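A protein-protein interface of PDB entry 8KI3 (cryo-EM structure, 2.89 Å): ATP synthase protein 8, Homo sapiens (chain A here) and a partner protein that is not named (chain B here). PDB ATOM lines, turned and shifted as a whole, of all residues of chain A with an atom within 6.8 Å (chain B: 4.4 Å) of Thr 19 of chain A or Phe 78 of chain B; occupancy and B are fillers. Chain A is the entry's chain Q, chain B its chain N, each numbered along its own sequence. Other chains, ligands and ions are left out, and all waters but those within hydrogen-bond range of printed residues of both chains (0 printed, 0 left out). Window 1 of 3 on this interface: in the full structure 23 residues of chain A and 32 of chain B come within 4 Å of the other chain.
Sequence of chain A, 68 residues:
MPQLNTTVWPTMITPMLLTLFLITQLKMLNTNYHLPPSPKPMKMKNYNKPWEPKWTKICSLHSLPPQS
O of Ile 24 of chain B is in hydrogen-bond range of OG1 of Thr 19 of chain A (3.5 Å).
The backbone NH of Gln 25 of chain A lies close to the side-chain hydroxyl of Ser 74 of chain B, at 3.4 Å.
OG1 of Thr 24 of chain A is in hydrogen-bond range of O of Thr 19 of chain A (2.7 Å).
The side-chain amide nitrogen (NE2) of Gln 25 of chain A lies within hydrogen-bond range of the backbone carbonyl oxygen (O) of Leu 20 of chain A (3.2 Å).
OG1 of Thr 19 of chain A lies within hydrogen-bond range of O of Pro 15 of chain A (3.2 Å).
Among the printed residues, merely in contact across the chains: Pro 15 of chain A with Ile 24 of chain B (3.4 Å), Pro 15 of chain A with Leu 25 of chain B (3.96 Å), Met 16 of chain A with Ile 24 of chain B (3.7 Å), Met 16 of chain A with Phe 78 of chain B (3.8 Å), Met 16 of chain A with Met 100 of chain B (3.6 Å), Met 16 of chain A with Met 104 of chain B (3.6 Å), Thr 19 of chain A with Leu 25 of chain B (3.2 Å), Thr 19 of chain A with Pro 28 of chain B (3.6 Å), Thr 19 of chain A with Phe 78 of chain B (3.6 Å), Leu 20 of chain A with Ser 74 of chain B (3.3 Å), Leu 20 of chain A with Leu 75 of chain B (3.7 Å), Leu 20 of chain A with Met 104 of chain B (3.9 Å), Ile 23 of chain A with Leu 25 of chain B (3.9 Å), Ile 23 of chain A with Pro 28 of chain B (3.5 Å), Thr 24 of chain A with Pro 28 of chain B (3.4 Å) and Thr 24 of chain A with Ser 74 of chain B (3.2 Å).
Printed residues of chain B within 4 Å of Met 16 of chain A: Ile 24, Phe 78, Met 100 and Met 104.
Of chain B, only Ile 24, Leu 25, Pro 28 and Phe 78 come within 4 Å of Thr 19 of chain A.
Of the printed residues of chain B, Ile 23 of chain A touches Leu 25 (3.9 Å) and Pro 28 (3.5 Å).
Of the printed residues of chain B, Thr 24 of chain A touches Pro 28 and Ser 74.
Phe 78 of chain B touches two residues of chain A.
The nearest printed residue of chain B that does not touch Thr 19 of chain A is Ser 74 of chain B (5.2 Å).
Of the 14 printed residues of chain B, 8 touch a printed residue of chain A.
Printed residues of chain A that touch a printed residue of chain B: Pro 15, Met 16, Thr 19, Leu 20, Ile 23, Thr 24 and Gln 25.
Hydrophobic or aromatic side chains of chain A that line the printed part of chain B: Pro 15, Met 16, Leu 20 and Ile 23.
Among the printed residues, 18 pairs touch across the chains.
Among the printed residues, no Asp or Glu carboxylate lies within 4 Å of a Lys or Arg side-chain nitrogen of the other chain.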
ATOM      1  N   THR A  14      -1.861 -32.364 -12.452  1.00  0.00           N
ATOM      2  CA  THR A  14      -1.332 -31.011 -12.564  1.00  0.00           C
ATOM      3  C   THR A  14      -0.645 -30.737 -13.902  1.00  0.00           C
ATOM      4  O   THR A  14      -0.863 -29.658 -14.465  1.00  0.00           O
ATOM      5  CB  THR A  14      -0.392 -30.694 -11.396  1.00  0.00           C
ATOM      6  OG1 THR A  14       0.917 -31.213 -11.651  1.00  0.00           O
ATOM      7  CG2 THR A  14      -0.930 -31.290 -10.113  1.00  0.00           C
ATOM      8  N   PRO A  15       0.170 -31.637 -14.467  1.00  0.00           N
ATOM      9  CA  PRO A  15       0.739 -31.335 -15.788  1.00  0.00           C
ATOM     10  C   PRO A  15      -0.277 -31.407 -16.906  1.00  0.00           C
ATOM     11  O   PRO A  15       0.009 -30.918 -18.005  1.00  0.00           O
ATOM     12  CB  PRO A  15       1.821 -32.399 -15.955  1.00  0.00           C
ATOM     13  CG  PRO A  15       1.305 -33.528 -15.224  1.00  0.00           C
ATOM     14  CD  PRO A  15       0.608 -32.968 -14.017  1.00  0.00           C
ATOM     15  N   MET A  16      -1.447 -31.996 -16.675  1.00  0.00           N
ATOM     16  CA  MET A  16      -2.524 -31.877 -17.648  1.00  0.00           C
ATOM     17  C   MET A  16      -3.117 -30.479 -17.616  1.00  0.00           C
ATOM     18  O   MET A  16      -3.234 -29.817 -18.653  1.00  0.00           O
ATOM     19  CB  MET A  16      -3.607 -32.917 -17.381  1.00  0.00           C
ATOM     20  CG  MET A  16      -4.615 -33.022 -18.501  1.00  0.00           C
ATOM     21  SD  MET A  16      -5.983 -31.873 -18.322  1.00  0.00           S
ATOM     22  CE  MET A  16      -6.627 -32.393 -16.749  1.00  0.00           C
ATOM     23  N   LEU A  17      -3.515 -30.018 -16.428  1.00  0.00           N
ATOM     24  CA  LEU A  17      -4.066 -28.674 -16.293  1.00  0.00           C
ATOM     25  C   LEU A  17      -3.108 -27.621 -16.823  1.00  0.00           C
ATOM     26  O   LEU A  17      -3.543 -26.614 -17.390  1.00  0.00           O
ATOM     27  CB  LEU A  17      -4.397 -28.390 -14.832  1.00  0.00           C
ATOM     28  CG  LEU A  17      -5.461 -29.269 -14.187  1.00  0.00           C
ATOM     29  CD1 LEU A  17      -5.546 -28.966 -12.709  1.00  0.00           C
ATOM     30  CD2 LEU A  17      -6.798 -29.053 -14.852  1.00  0.00           C
ATOM     31  N   LEU A  18      -1.805 -27.835 -16.653  1.00  0.00           N
ATOM     32  CA  LEU A  18      -0.815 -26.913 -17.186  1.00  0.00           C
ATOM     33  C   LEU A  18      -0.680 -27.008 -18.696  1.00  0.00           C
ATOM     34  O   LEU A  18       0.049 -26.205 -19.284  1.00  0.00           O
ATOM     35  CB  LEU A  18       0.539 -27.177 -16.533  1.00  0.00           C
ATOM     36  CG  LEU A  18       1.545 -26.032 -16.539  1.00  0.00           C
ATOM     37  CD1 LEU A  18       1.084 -24.938 -15.600  1.00  0.00           C
ATOM     38  CD2 LEU A  18       2.917 -26.542 -16.147  1.00  0.00           C
ATOM     39  N   THR A  19      -1.352 -27.962 -19.336  1.00  0.00           N
ATOM     40  CA  THR A  19      -1.315 -28.121 -20.782  1.00  0.00           C
ATOM     41  C   THR A  19      -2.656 -27.838 -21.436  1.00  0.00           C
ATOM     42  O   THR A  19      -2.726 -27.090 -22.412  1.00  0.00           O
ATOM     43  CB  THR A  19      -0.859 -29.539 -21.144  1.00  0.00           C
ATOM     44  OG1 THR A  19       0.551 -29.653 -20.940  1.00  0.00           O
ATOM     45  CG2 THR A  19      -1.170 -29.845 -22.586  1.00  0.00           C
ATOM     46  N   LEU A  20      -3.734 -28.415 -20.912  1.00  0.00           N
ATOM     47  CA  LEU A  20      -5.035 -28.219 -21.529  1.00  0.00           C
ATOM     48  C   LEU A  20      -5.523 -26.790 -21.365  1.00  0.00           C
ATOM     49  O   LEU A  20      -6.298 -26.304 -22.193  1.00  0.00           O
ATOM     50  CB  LEU A  20      -6.042 -29.198 -20.933  1.00  0.00           C
ATOM     51  CG  LEU A  20      -7.483 -29.103 -21.421  1.00  0.00           C
ATOM     52  CD1 LEU A  20      -7.529 -29.226 -22.921  1.00  0.00           C
ATOM     53  CD2 LEU A  20      -8.337 -30.164 -20.772  1.00  0.00           C
ATOM     54  N   PHE A  21      -5.069 -26.094 -20.323  1.00  0.00           N
ATOM     55  CA  PHE A  21      -5.618 -24.790 -19.982  1.00  0.00           C
ATOM     56  C   PHE A  21      -4.660 -23.626 -20.178  1.00  0.00           C
ATOM     57  O   PHE A  21      -5.120 -22.486 -20.248  1.00  0.00           O
ATOM     58  CB  PHE A  21      -6.101 -24.785 -18.525  1.00  0.00           C
ATOM     59  CG  PHE A  21      -7.357 -25.562 -18.307  1.00  0.00           C
ATOM     60  CD1 PHE A  21      -8.578 -25.039 -18.669  1.00  0.00           C
ATOM     61  CD2 PHE A  21      -7.318 -26.821 -17.749  1.00  0.00           C
ATOM     62  CE1 PHE A  21      -9.735 -25.754 -18.472  1.00  0.00           C
ATOM     63  CE2 PHE A  21      -8.475 -27.542 -17.552  1.00  0.00           C
ATOM     64  CZ  PHE A  21      -9.684 -27.008 -17.913  1.00  0.00           C
ATOM     65  N   LEU A  22      -3.364 -23.866 -20.266  1.00  0.00           N
ATOM     66  CA  LEU A  22      -2.435 -22.753 -20.385  1.00  0.00           C
ATOM     67  C   LEU A  22      -1.508 -22.855 -21.579  1.00  0.00           C
ATOM     68  O   LEU A  22      -1.187 -21.833 -22.179  1.00  0.00           O
ATOM     69  CB  LEU A  22      -1.601 -22.621 -19.107  1.00  0.00           C
ATOM     70  CG  LEU A  22      -0.707 -21.387 -18.980  1.00  0.00           C
ATOM     71  CD1 LEU A  22      -0.714 -20.891 -17.553  1.00  0.00           C
ATOM     72  CD2 LEU A  22       0.714 -21.693 -19.406  1.00  0.00           C
ATOM     73  N   ILE A  23      -1.054 -24.049 -21.940  1.00  0.00           N
ATOM     74  CA  ILE A  23      -0.062 -24.159 -23.002  1.00  0.00           C
ATOM     75  C   ILE A  23      -0.709 -24.459 -24.343  1.00  0.00           C
ATOM     76  O   ILE A  23      -0.296 -23.915 -25.367  1.00  0.00           O
ATOM     77  CB  ILE A  23       0.993 -25.215 -22.632  1.00  0.00           C
ATOM     78  CG1 ILE A  23       1.830 -24.731 -21.456  1.00  0.00           C
ATOM     79  CG2 ILE A  23       1.907 -25.477 -23.794  1.00  0.00           C
ATOM     80  CD1 ILE A  23       2.971 -25.646 -21.118  1.00  0.00           C
ATOM     81  N   THR A  24      -1.730 -25.314 -24.379  1.00  0.00           N
ATOM     82  CA  THR A  24      -2.374 -25.598 -25.656  1.00  0.00           C
ATOM     83  C   THR A  24      -3.234 -24.429 -26.103  1.00  0.00           C
ATOM     84  O   THR A  24      -3.305 -24.128 -27.298  1.00  0.00           O
ATOM     85  CB  THR A  24      -3.219 -26.862 -25.569  1.00  0.00           C
ATOM     86  OG1 THR A  24      -2.443 -27.915 -24.992  1.00  0.00           O
ATOM     87  CG2 THR A  24      -3.653 -27.282 -26.952  1.00  0.00           C
ATOM     88  N   GLN A  25      -3.896 -23.760 -25.161  1.00  0.00           N
ATOM     89  CA  GLN A  25      -4.725 -22.618 -25.522  1.00  0.00           C
ATOM     90  C   GLN A  25      -3.876 -21.442 -25.975  1.00  0.00           C
ATOM     91  O   GLN A  25      -4.202 -20.786 -26.969  1.00  0.00           O
ATOM     92  CB  GLN A  25      -5.611 -22.225 -24.348  1.00  0.00           C
ATOM     93  CG  GLN A  25      -6.492 -23.350 -23.868  1.00  0.00           C
ATOM     94  CD  GLN A  25      -7.595 -22.870 -22.961  1.00  0.00           C
ATOM     95  OE1 GLN A  25      -7.893 -21.681 -22.903  1.00  0.00           O
ATOM     96  NE2 GLN A  25      -8.210 -23.795 -22.241  1.00  0.00           N
ATOM     97  N   LEU A  26      -2.788 -21.155 -25.257  1.00  0.00           N
ATOM     98  CA  LEU A  26      -1.884 -20.085 -25.668  1.00  0.00           C
ATOM     99  C   LEU A  26      -1.445 -20.257 -27.111  1.00  0.00           C
ATOM    100  O   LEU A  26      -1.336 -19.279 -27.855  1.00  0.00           O
ATOM    101  CB  LEU A  26      -0.666 -20.044 -24.753  1.00  0.00           C
ATOM    102  CG  LEU A  26      -0.691 -18.981 -23.665  1.00  0.00           C
ATOM    103  CD1 LEU A  26       0.516 -19.130 -22.771  1.00  0.00           C
ATOM    104  CD2 LEU A  26      -0.720 -17.614 -24.294  1.00  0.00           C
ATOM    105  N   ILE B  24       3.102 -35.516 -20.836  1.00  0.00           N
ATOM    106  CA  ILE B  24       1.833 -34.810 -20.922  1.00  0.00           C
ATOM    107  C   ILE B  24       2.025 -33.416 -21.503  1.00  0.00           C
ATOM    108  O   ILE B  24       1.119 -32.879 -22.149  1.00  0.00           O
ATOM    109  CB  ILE B  24       1.166 -34.766 -19.538  1.00  0.00           C
ATOM    110  CG1 ILE B  24       0.833 -36.180 -19.074  1.00  0.00           C
ATOM    111  CG2 ILE B  24      -0.098 -33.950 -19.572  1.00  0.00           C
ATOM    112  CD1 ILE B  24       0.169 -36.236 -17.732  1.00  0.00           C
ATOM    113  N   LEU B  25       3.197 -32.818 -21.317  1.00  0.00           N
ATOM    114  CA  LEU B  25       3.467 -31.477 -21.817  1.00  0.00           C
ATOM    115  C   LEU B  25       4.012 -31.466 -23.239  1.00  0.00           C
ATOM    116  O   LEU B  25       4.241 -30.385 -23.787  1.00  0.00           O
ATOM    117  CB  LEU B  25       4.454 -30.762 -20.891  1.00  0.00           C
ATOM    118  CG  LEU B  25       4.006 -30.460 -19.462  1.00  0.00           C
ATOM    119  CD1 LEU B  25       5.203 -30.407 -18.539  1.00  0.00           C
ATOM    120  CD2 LEU B  25       3.259 -29.151 -19.411  1.00  0.00           C
ATOM    121  N   PRO B  28       1.628 -30.155 -27.033  1.00  0.00           N
ATOM    122  CA  PRO B  28       1.671 -28.782 -27.560  1.00  0.00           C
ATOM    123  C   PRO B  28       2.946 -28.443 -28.307  1.00  0.00           C
ATOM    124  O   PRO B  28       2.967 -27.434 -29.015  1.00  0.00           O
ATOM    125  CB  PRO B  28       1.527 -27.915 -26.307  1.00  0.00           C
ATOM    126  CG  PRO B  28       0.880 -28.774 -25.335  1.00  0.00           C
ATOM    127  CD  PRO B  28       1.453 -30.126 -25.571  1.00  0.00           C
ATOM    128  N   SER B  74      -9.265 -26.274 -28.199  1.00  0.00           N
ATOM    129  CA  SER B  74      -8.018 -26.647 -27.558  1.00  0.00           C
ATOM    130  C   SER B  74      -8.141 -27.863 -26.741  1.00  0.00           C
ATOM    131  O   SER B  74      -7.186 -28.192 -26.047  1.00  0.00           O
ATOM    132  CB  SER B  74      -7.506 -25.509 -26.688  1.00  0.00           C
ATOM    133  OG  SER B  74      -6.409 -25.942 -25.915  1.00  0.00           O
ATOM    134  N   LEU B  75      -9.285 -28.541 -26.770  1.00  0.00           N
ATOM    135  CA  LEU B  75      -9.471 -29.818 -26.099  1.00  0.00           C
ATOM    136  C   LEU B  75      -9.499 -30.982 -27.070  1.00  0.00           C
ATOM    137  O   LEU B  75      -8.942 -32.040 -26.779  1.00  0.00           O
ATOM    138  CB  LEU B  75     -10.768 -29.807 -25.291  1.00  0.00           C
ATOM    139  CG  LEU B  75     -11.246 -31.140 -24.737  1.00  0.00           C
ATOM    140  CD1 LEU B  75     -10.373 -31.559 -23.588  1.00  0.00           C
ATOM    141  CD2 LEU B  75     -12.678 -31.023 -24.298  1.00  0.00           C
ATOM    142  N   ILE B  76     -10.138 -30.810 -28.229  1.00  0.00           N
ATOM    143  CA  ILE B  76     -10.049 -31.816 -29.270  1.00  0.00           C
ATOM    144  C   ILE B  76      -8.646 -31.879 -29.844  1.00  0.00           C
ATOM    145  O   ILE B  76      -8.278 -32.880 -30.461  1.00  0.00           O
ATOM    146  CB  ILE B  76     -11.076 -31.535 -30.376  1.00  0.00           C
ATOM    147  CG1 ILE B  76     -11.240 -32.748 -31.282  1.00  0.00           C
ATOM    148  CG2 ILE B  76     -10.657 -30.349 -31.189  1.00  0.00           C
ATOM    149  CD1 ILE B  76     -12.160 -32.502 -32.441  1.00  0.00           C
ATOM    150  N   ILE B  77      -7.846 -30.835 -29.648  1.00  0.00           N
ATOM    151  CA  ILE B  77      -6.475 -30.852 -30.134  1.00  0.00           C
ATOM    152  C   ILE B  77      -5.561 -31.535 -29.130  1.00  0.00           C
ATOM    153  O   ILE B  77      -4.545 -32.124 -29.508  1.00  0.00           O
ATOM    154  CB  ILE B  77      -6.019 -29.419 -30.452  1.00  0.00           C
ATOM    155  CG1 ILE B  77      -6.722 -28.906 -31.703  1.00  0.00           C
ATOM    156  CG2 ILE B  77      -4.546 -29.357 -30.669  1.00  0.00           C
ATOM    157  CD1 ILE B  77      -6.550 -29.796 -32.901  1.00  0.00           C
ATOM    158  N   PHE B  78      -5.916 -31.508 -27.849  1.00  0.00           N
ATOM    159  CA  PHE B  78      -5.101 -32.147 -26.826  1.00  0.00           C
ATOM    160  C   PHE B  78      -5.438 -33.618 -26.637  1.00  0.00           C
ATOM    161  O   PHE B  78      -4.565 -34.396 -26.241  1.00  0.00           O
ATOM    162  CB  PHE B  78      -5.252 -31.411 -25.495  1.00  0.00           C
ATOM    163  CG  PHE B  78      -4.685 -32.152 -24.329  1.00  0.00           C
ATOM    164  CD1 PHE B  78      -3.323 -32.283 -24.174  1.00  0.00           C
ATOM    165  CD2 PHE B  78      -5.514 -32.723 -23.388  1.00  0.00           C
ATOM    166  CE1 PHE B  78      -2.801 -32.967 -23.101  1.00  0.00           C
ATOM    167  CE2 PHE B  78      -4.995 -33.407 -22.315  1.00  0.00           C
ATOM    168  CZ  PHE B  78      -3.640 -33.529 -22.172  1.00  0.00           C
ATOM    169  N   ILE B  79      -6.673 -34.028 -26.911  1.00  0.00           N
ATOM    170  CA  ILE B  79      -7.002 -35.443 -26.805  1.00  0.00           C
ATOM    171  C   ILE B  79      -6.644 -36.178 -28.088  1.00  0.00           C
ATOM    172  O   ILE B  79      -6.217 -37.334 -28.053  1.00  0.00           O
ATOM    173  CB  ILE B  79      -8.483 -35.628 -26.447  1.00  0.00           C
ATOM    174  CG1 ILE B  79      -8.810 -34.913 -25.148  1.00  0.00           C
ATOM    175  CG2 ILE B  79      -8.802 -37.085 -26.284  1.00  0.00           C
ATOM    176  CD1 ILE B  79     -10.242 -35.063 -24.747  1.00  0.00           C
ATOM    177  N   ALA B  80      -6.807 -35.531 -29.242  1.00  0.00           N
ATOM    178  CA  ALA B  80      -6.458 -36.191 -30.492  1.00  0.00           C
ATOM    179  C   ALA B  80      -4.957 -36.288 -30.688  1.00  0.00           C
ATOM    180  O   ALA B  80      -4.506 -37.079 -31.517  1.00  0.00           O
ATOM    181  CB  ALA B  80      -7.082 -35.465 -31.677  1.00  0.00           C
ATOM    182  N   THR B  81      -4.176 -35.505 -29.954  1.00  0.00           N
ATOM    183  CA  THR B  81      -2.729 -35.600 -30.033  1.00  0.00           C
ATOM    184  C   THR B  81      -2.146 -36.483 -28.945  1.00  0.00           C
ATOM    185  O   THR B  81      -1.063 -37.045 -29.135  1.00  0.00           O
ATOM    186  CB  THR B  81      -2.102 -34.209 -29.949  1.00  0.00           C
ATOM    187  OG1 THR B  81      -2.771 -33.334 -30.860  1.00  0.00           O
ATOM    188  CG2 THR B  81      -0.646 -34.265 -30.323  1.00  0.00           C
ATOM    189  N   THR B  82      -2.839 -36.632 -27.819  1.00  0.00           N
ATOM    190  CA  THR B  82      -2.378 -37.554 -26.793  1.00  0.00           C
ATOM    191  C   THR B  82      -2.654 -38.997 -27.186  1.00  0.00           C
ATOM    192  O   THR B  82      -1.827 -39.878 -26.940  1.00  0.00           O
ATOM    193  CB  THR B  82      -3.047 -37.240 -25.464  1.00  0.00           C
ATOM    194  OG1 THR B  82      -3.067 -35.825 -25.273  1.00  0.00           O
ATOM    195  CG2 THR B  82      -2.272 -37.863 -24.345  1.00  0.00           C
ATOM    196  N   MET B 100      -6.293 -38.609 -15.062  1.00  0.00           N
ATOM    197  CA  MET B 100      -6.303 -37.527 -16.040  1.00  0.00           C
ATOM    198  C   MET B 100      -7.685 -37.353 -16.652  1.00  0.00           C
ATOM    199  O   MET B 100      -8.209 -36.237 -16.718  1.00  0.00           O
ATOM    200  CB  MET B 100      -5.266 -37.798 -17.125  1.00  0.00           C
ATOM    201  CG  MET B 100      -4.569 -36.563 -17.624  1.00  0.00           C
ATOM    202  SD  MET B 100      -3.743 -36.836 -19.192  1.00  0.00           S
ATOM    203  CE  MET B 100      -5.143 -36.855 -20.298  1.00  0.00           C
ATOM    204  N   MET B 104     -10.222 -34.026 -16.846  1.00  0.00           N
ATOM    205  CA  MET B 104     -10.746 -33.327 -18.010  1.00  0.00           C
ATOM    206  C   MET B 104     -12.263 -33.358 -18.069  1.00  0.00           C
ATOM    207  O   MET B 104     -12.860 -32.535 -18.768  1.00  0.00           O
ATOM    208  CB  MET B 104     -10.199 -33.937 -19.299  1.00  0.00           C
ATOM    209  CG  MET B 104      -8.712 -33.840 -19.469  1.00  0.00           C
ATOM    210  SD  MET B 104      -8.221 -34.279 -21.142  1.00  0.00           S
ATOM    211  CE  MET B 104      -8.780 -35.970 -21.216  1.00  0.00           C
